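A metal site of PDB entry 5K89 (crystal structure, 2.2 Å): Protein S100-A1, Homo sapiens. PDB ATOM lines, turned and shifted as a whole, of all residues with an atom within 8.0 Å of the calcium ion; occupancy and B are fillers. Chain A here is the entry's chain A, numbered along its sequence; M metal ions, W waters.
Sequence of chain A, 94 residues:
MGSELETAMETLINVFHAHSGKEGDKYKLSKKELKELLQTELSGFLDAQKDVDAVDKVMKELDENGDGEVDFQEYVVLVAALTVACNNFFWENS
The side-chain hydroxyl (OG) of Ser 30 is in hydrogen-bond range of the backbone NH (N) of Glu 33.
The side-chain hydroxyl (OG) of Ser 20 lies within hydrogen-bond range of the backbone carbonyl oxygen (O) of Lys 26, 2.8 Å away.
N of Lys 22 lies close to OE1 of Glu 33.
OD1 of Asp 25 sits at hydrogen-bond distance from N of Tyr 27 (2.8 Å).
N of Tyr 27 lies close to OG of Ser 20, at 3.4 Å.
Of the 19 residues printed, 5 come within 4 Å of the calcium ion.
The nearest printed residue that does not touch the calcium ion is Gly 24 (4.2 Å).
The calcium ion is bound by water W1 (2.2 Å), the side-chain carboxylate (OE2) of Glu 33 (2.3 Å), the backbone carbonyl oxygen (O) of Glu 23 (2.4 Å), the backbone carbonyl oxygen (O) of Ser 20 (2.4 Å), the backbone carbonyl oxygen (O) of Asp 25 (2.5 Å), the backbone carbonyl oxygen (O) of Lys 28 (2.6 Å) and the side-chain carboxylate (OE1) of Glu 33 (2.6 Å).
The calcium ion has seven donor atoms within binding distance.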
ATOM      1  N   PHE A  16     -14.454 -14.707  23.355  1.00  0.00           N
ATOM      2  CA  PHE A  16     -14.833 -15.306  22.102  1.00  0.00           C
ATOM      3  C   PHE A  16     -15.146 -16.760  22.245  1.00  0.00           C
ATOM      4  O   PHE A  16     -16.089 -17.249  21.680  1.00  0.00           O
ATOM      5  CB  PHE A  16     -13.720 -15.183  21.099  1.00  0.00           C
ATOM      6  CG  PHE A  16     -13.933 -15.987  19.872  1.00  0.00           C
ATOM      7  CD1 PHE A  16     -14.383 -15.399  18.732  1.00  0.00           C
ATOM      8  CD2 PHE A  16     -13.681 -17.317  19.865  1.00  0.00           C
ATOM      9  CE1 PHE A  16     -14.590 -16.141  17.602  1.00  0.00           C
ATOM     10  CE2 PHE A  16     -13.871 -18.069  18.744  1.00  0.00           C
ATOM     11  CZ  PHE A  16     -14.326 -17.473  17.602  1.00  0.00           C
ATOM     12  N   HIS A  17     -14.339 -17.463  23.029  1.00  0.00           N
ATOM     13  CA  HIS A  17     -14.529 -18.876  23.300  1.00  0.00           C
ATOM     14  C   HIS A  17     -15.743 -19.146  24.149  1.00  0.00           C
ATOM     15  O   HIS A  17     -16.340 -20.184  24.049  1.00  0.00           O
ATOM     16  CB  HIS A  17     -13.240 -19.552  23.746  1.00  0.00           C
ATOM     17  CG  HIS A  17     -12.284 -19.738  22.632  1.00  0.00           C
ATOM     18  ND1 HIS A  17     -11.143 -18.973  22.496  1.00  0.00           N
ATOM     19  CD2 HIS A  17     -12.311 -20.553  21.554  1.00  0.00           C
ATOM     20  CE1 HIS A  17     -10.507 -19.323  21.404  1.00  0.00           C
ATOM     21  NE2 HIS A  17     -11.196 -20.277  20.811  1.00  0.00           N
ATOM     22  N   HIS A  19     -18.639 -17.769  23.757  1.00  0.00           N
ATOM     23  CA  HIS A  19     -19.822 -17.876  22.948  1.00  0.00           C
ATOM     24  C   HIS A  19     -19.622 -18.802  21.750  1.00  0.00           C
ATOM     25  O   HIS A  19     -20.554 -19.367  21.233  1.00  0.00           O
ATOM     26  CB  HIS A  19     -20.309 -16.483  22.541  1.00  0.00           C
ATOM     27  CG  HIS A  19     -20.432 -15.555  23.702  1.00  0.00           C
ATOM     28  ND1 HIS A  19     -21.471 -15.625  24.599  1.00  0.00           N
ATOM     29  CD2 HIS A  19     -19.630 -14.554  24.131  1.00  0.00           C
ATOM     30  CE1 HIS A  19     -21.306 -14.703  25.530  1.00  0.00           C
ATOM     31  NE2 HIS A  19     -20.200 -14.043  25.266  1.00  0.00           N
ATOM     32  N   SER A  20     -18.378 -18.969  21.334  1.00  0.00           N
ATOM     33  CA  SER A  20     -18.067 -19.847  20.200  1.00  0.00           C
ATOM     34  C   SER A  20     -18.345 -21.320  20.511  1.00  0.00           C
ATOM     35  O   SER A  20     -18.608 -22.105  19.589  1.00  0.00           O
ATOM     36  CB  SER A  20     -16.604 -19.675  19.817  1.00  0.00           C
ATOM     37  OG  SER A  20     -16.241 -20.530  18.758  1.00  0.00           O
ATOM     38  N   GLY A  21     -18.274 -21.726  21.769  1.00  0.00           N
ATOM     39  CA  GLY A  21     -18.364 -23.142  22.049  1.00  0.00           C
ATOM     40  C   GLY A  21     -19.749 -23.614  22.429  1.00  0.00           C
ATOM     41  O   GLY A  21     -19.879 -24.631  23.115  1.00  0.00           O
ATOM     42  N   LYS A  22     -20.773 -22.908  21.983  1.00  0.00           N
ATOM     43  CA  LYS A  22     -22.138 -23.256  22.390  1.00  0.00           C
ATOM     44  C   LYS A  22     -22.812 -24.264  21.459  1.00  0.00           C
ATOM     45  O   LYS A  22     -23.607 -25.075  21.946  1.00  0.00           O
ATOM     46  CB  LYS A  22     -23.016 -22.001  22.481  1.00  0.00           C
ATOM     47  CG  LYS A  22     -22.547 -20.958  23.483  1.00  0.00           C
ATOM     48  CD  LYS A  22     -22.580 -21.497  24.895  1.00  0.00           C
ATOM     49  CE  LYS A  22     -22.280 -20.395  25.897  1.00  0.00           C
ATOM     50  NZ  LYS A  22     -23.241 -19.269  25.777  1.00  0.00           N
ATOM     51  N   GLU A  23     -22.540 -24.216  20.159  1.00  0.00           N
ATOM     52  CA  GLU A  23     -23.057 -25.210  19.213  1.00  0.00           C
ATOM     53  C   GLU A  23     -22.284 -25.096  17.907  1.00  0.00           C
ATOM     54  O   GLU A  23     -21.658 -24.073  17.610  1.00  0.00           O
ATOM     55  CB  GLU A  23     -24.564 -25.066  18.945  1.00  0.00           C
ATOM     56  CG  GLU A  23     -25.522 -25.967  19.794  1.00  0.00           C
ATOM     57  CD  GLU A  23     -25.377 -27.494  19.571  1.00  0.00           C
ATOM     58  OE1 GLU A  23     -24.907 -28.220  20.488  1.00  0.00           O
ATOM     59  OE2 GLU A  23     -25.768 -27.972  18.476  1.00  0.00           O
ATOM     60  N   GLY A  24     -22.345 -26.172  17.131  1.00  0.00           N
ATOM     61  CA  GLY A  24     -21.572 -26.309  15.906  1.00  0.00           C
ATOM     62  C   GLY A  24     -20.077 -26.332  16.185  1.00  0.00           C
ATOM     63  O   GLY A  24     -19.591 -26.942  17.149  1.00  0.00           O
ATOM     64  N   ASP A  25     -19.341 -25.636  15.329  1.00  0.00           N
ATOM     65  CA  ASP A  25     -17.892 -25.568  15.448  1.00  0.00           C
ATOM     66  C   ASP A  25     -17.543 -24.796  16.715  1.00  0.00           C
ATOM     67  O   ASP A  25     -17.882 -23.603  16.829  1.00  0.00           O
ATOM     68  CB  ASP A  25     -17.302 -24.901  14.213  1.00  0.00           C
ATOM     69  CG  ASP A  25     -15.804 -25.085  14.086  1.00  0.00           C
ATOM     70  OD1 ASP A  25     -15.088 -24.916  15.096  1.00  0.00           O
ATOM     71  OD2 ASP A  25     -15.335 -25.381  12.972  1.00  0.00           O
ATOM     72  N   LYS A  26     -16.881 -25.452  17.673  1.00  0.00           N
ATOM     73  CA  LYS A  26     -16.481 -24.803  18.916  1.00  0.00           C
ATOM     74  C   LYS A  26     -15.496 -23.652  18.710  1.00  0.00           C
ATOM     75  O   LYS A  26     -15.199 -22.923  19.660  1.00  0.00           O
ATOM     76  CB  LYS A  26     -15.862 -25.827  19.881  1.00  0.00           C
ATOM     77  CG  LYS A  26     -16.867 -26.662  20.685  1.00  0.00           C
ATOM     78  CD  LYS A  26     -16.325 -26.999  22.081  1.00  0.00           C
ATOM     79  CE  LYS A  26     -17.415 -26.881  23.152  1.00  0.00           C
ATOM     80  NZ  LYS A  26     -16.904 -26.252  24.411  1.00  0.00           N
ATOM     81  N   TYR A  27     -14.968 -23.474  17.499  1.00  0.00           N
ATOM     82  CA  TYR A  27     -13.984 -22.437  17.219  1.00  0.00           C
ATOM     83  C   TYR A  27     -14.497 -21.430  16.175  1.00  0.00           C
ATOM     84  O   TYR A  27     -13.695 -20.741  15.539  1.00  0.00           O
ATOM     85  CB  TYR A  27     -12.669 -23.086  16.765  1.00  0.00           C
ATOM     86  CG  TYR A  27     -12.021 -24.071  17.747  1.00  0.00           C
ATOM     87  CD1 TYR A  27     -12.190 -25.441  17.619  1.00  0.00           C
ATOM     88  CD2 TYR A  27     -11.213 -23.614  18.786  1.00  0.00           C
ATOM     89  CE1 TYR A  27     -11.587 -26.341  18.499  1.00  0.00           C
ATOM     90  CE2 TYR A  27     -10.615 -24.492  19.664  1.00  0.00           C
ATOM     91  CZ  TYR A  27     -10.801 -25.844  19.516  1.00  0.00           C
ATOM     92  OH  TYR A  27     -10.196 -26.715  20.399  1.00  0.00           O
ATOM     93  N   LYS A  28     -15.827 -21.334  16.003  1.00  0.00           N
ATOM     94  CA  LYS A  28     -16.489 -20.397  15.091  1.00  0.00           C
ATOM     95  C   LYS A  28     -17.837 -19.979  15.677  1.00  0.00           C
ATOM     96  O   LYS A  28     -18.576 -20.822  16.216  1.00  0.00           O
ATOM     97  CB  LYS A  28     -16.739 -21.026  13.714  1.00  0.00           C
ATOM     98  CG  LYS A  28     -15.487 -21.320  12.908  1.00  0.00           C
ATOM     99  CD  LYS A  28     -15.787 -22.323  11.830  1.00  0.00           C
ATOM    100  CE  LYS A  28     -15.695 -21.702  10.466  1.00  0.00           C
ATOM    101  NZ  LYS A  28     -15.854 -22.727   9.408  1.00  0.00           N
ATOM    102  N   LEU A  29     -18.160 -18.693  15.551  1.00  0.00           N
ATOM    103  CA  LEU A  29     -19.435 -18.150  16.023  1.00  0.00           C
ATOM    104  C   LEU A  29     -20.503 -18.298  14.933  1.00  0.00           C
ATOM    105  O   LEU A  29     -20.335 -17.774  13.835  1.00  0.00           O
ATOM    106  CB  LEU A  29     -19.282 -16.672  16.386  1.00  0.00           C
ATOM    107  CG  LEU A  29     -18.527 -16.325  17.655  1.00  0.00           C
ATOM    108  CD1 LEU A  29     -18.153 -14.865  17.671  1.00  0.00           C
ATOM    109  CD2 LEU A  29     -19.390 -16.655  18.844  1.00  0.00           C
ATOM    110  N   SER A  30     -21.589 -19.015  15.250  1.00  0.00           N
ATOM    111  CA  SER A  30     -22.737 -19.074  14.360  1.00  0.00           C
ATOM    112  C   SER A  30     -23.579 -17.814  14.506  1.00  0.00           C
ATOM    113  O   SER A  30     -23.301 -16.936  15.337  1.00  0.00           O
ATOM    114  CB  SER A  30     -23.595 -20.305  14.668  1.00  0.00           C
ATOM    115  OG  SER A  30     -24.385 -20.066  15.819  1.00  0.00           O
ATOM    116  N   LYS A  31     -24.639 -17.719  13.705  1.00  0.00           N
ATOM    117  CA  LYS A  31     -25.511 -16.551  13.717  1.00  0.00           C
ATOM    118  C   LYS A  31     -26.169 -16.352  15.076  1.00  0.00           C
ATOM    119  O   LYS A  31     -26.272 -15.233  15.570  1.00  0.00           O
ATOM    120  CB  LYS A  31     -26.577 -16.662  12.618  1.00  0.00           C
ATOM    121  CG  LYS A  31     -27.614 -15.551  12.650  1.00  0.00           C
ATOM    122  CD  LYS A  31     -28.509 -15.602  11.419  1.00  0.00           C
ATOM    123  CE  LYS A  31     -29.253 -14.290  11.222  1.00  0.00           C
ATOM    124  NZ  LYS A  31     -30.214 -14.366  10.091  1.00  0.00           N
ATOM    125  N   GLU A  33     -24.993 -17.628  17.952  1.00  0.00           N
ATOM    126  CA  GLU A  33     -23.929 -17.369  18.930  1.00  0.00           C
ATOM    127  C   GLU A  33     -23.431 -15.937  18.831  1.00  0.00           C
ATOM    128  O   GLU A  33     -23.039 -15.345  19.851  1.00  0.00           O
ATOM    129  CB  GLU A  33     -22.756 -18.328  18.740  1.00  0.00           C
ATOM    130  CG  GLU A  33     -23.058 -19.803  18.946  1.00  0.00           C
ATOM    131  CD  GLU A  33     -21.841 -20.679  18.726  1.00  0.00           C
ATOM    132  OE1 GLU A  33     -21.711 -21.695  19.442  1.00  0.00           O
ATOM    133  OE2 GLU A  33     -21.012 -20.369  17.848  1.00  0.00           O
ATOM    134  N   LEU A  34     -23.359 -15.407  17.612  1.00  0.00           N
ATOM    135  CA  LEU A  34     -22.946 -14.015  17.418  1.00  0.00           C
ATOM    136  C   LEU A  34     -23.945 -13.064  18.048  1.00  0.00           C
ATOM    137  O   LEU A  34     -23.565 -12.054  18.655  1.00  0.00           O
ATOM    138  CB  LEU A  34     -22.794 -13.751  15.923  1.00  0.00           C
ATOM    139  CG  LEU A  34     -22.444 -12.340  15.432  1.00  0.00           C
ATOM    140  CD1 LEU A  34     -20.988 -12.101  15.780  1.00  0.00           C
ATOM    141  CD2 LEU A  34     -22.676 -12.202  13.936  1.00  0.00           C
ATOM    142  N   GLU A  69     -20.131 -18.194   9.297  1.00  0.00           N
ATOM    143  CA  GLU A  69     -19.748 -18.159  10.700  1.00  0.00           C
ATOM    144  C   GLU A  69     -18.535 -17.252  10.873  1.00  0.00           C
ATOM    145  O   GLU A  69     -17.775 -17.036   9.930  1.00  0.00           O
ATOM    146  CB  GLU A  69     -19.434 -19.576  11.239  1.00  0.00           C
ATOM    147  CG  GLU A  69     -20.637 -20.529  11.391  1.00  0.00           C
ATOM    148  CD  GLU A  69     -20.310 -21.775  12.218  1.00  0.00           C
ATOM    149  OE1 GLU A  69     -20.239 -22.891  11.650  1.00  0.00           O
ATOM    150  OE2 GLU A  69     -20.109 -21.648  13.444  1.00  0.00           O
ATOM    151  N   VAL A  70     -18.387 -16.681  12.065  1.00  0.00           N
ATOM    152  CA  VAL A  70     -17.251 -15.830  12.376  1.00  0.00           C
ATOM    153  C   VAL A  70     -16.239 -16.635  13.189  1.00  0.00           C
ATOM    154  O   VAL A  70     -16.533 -17.077  14.301  1.00  0.00           O
ATOM    155  CB  VAL A  70     -17.653 -14.581  13.155  1.00  0.00           C
ATOM    156  CG1 VAL A  70     -16.394 -13.793  13.554  1.00  0.00           C
ATOM    157  CG2 VAL A  70     -18.601 -13.710  12.334  1.00  0.00           C
HETATM  158 CA    CA M   1     -19.965 -22.437  17.656  1.00  0.00          CA
HETATM  159  O   HOH W   1     -20.349 -22.828  15.504  1.00  0.00           O
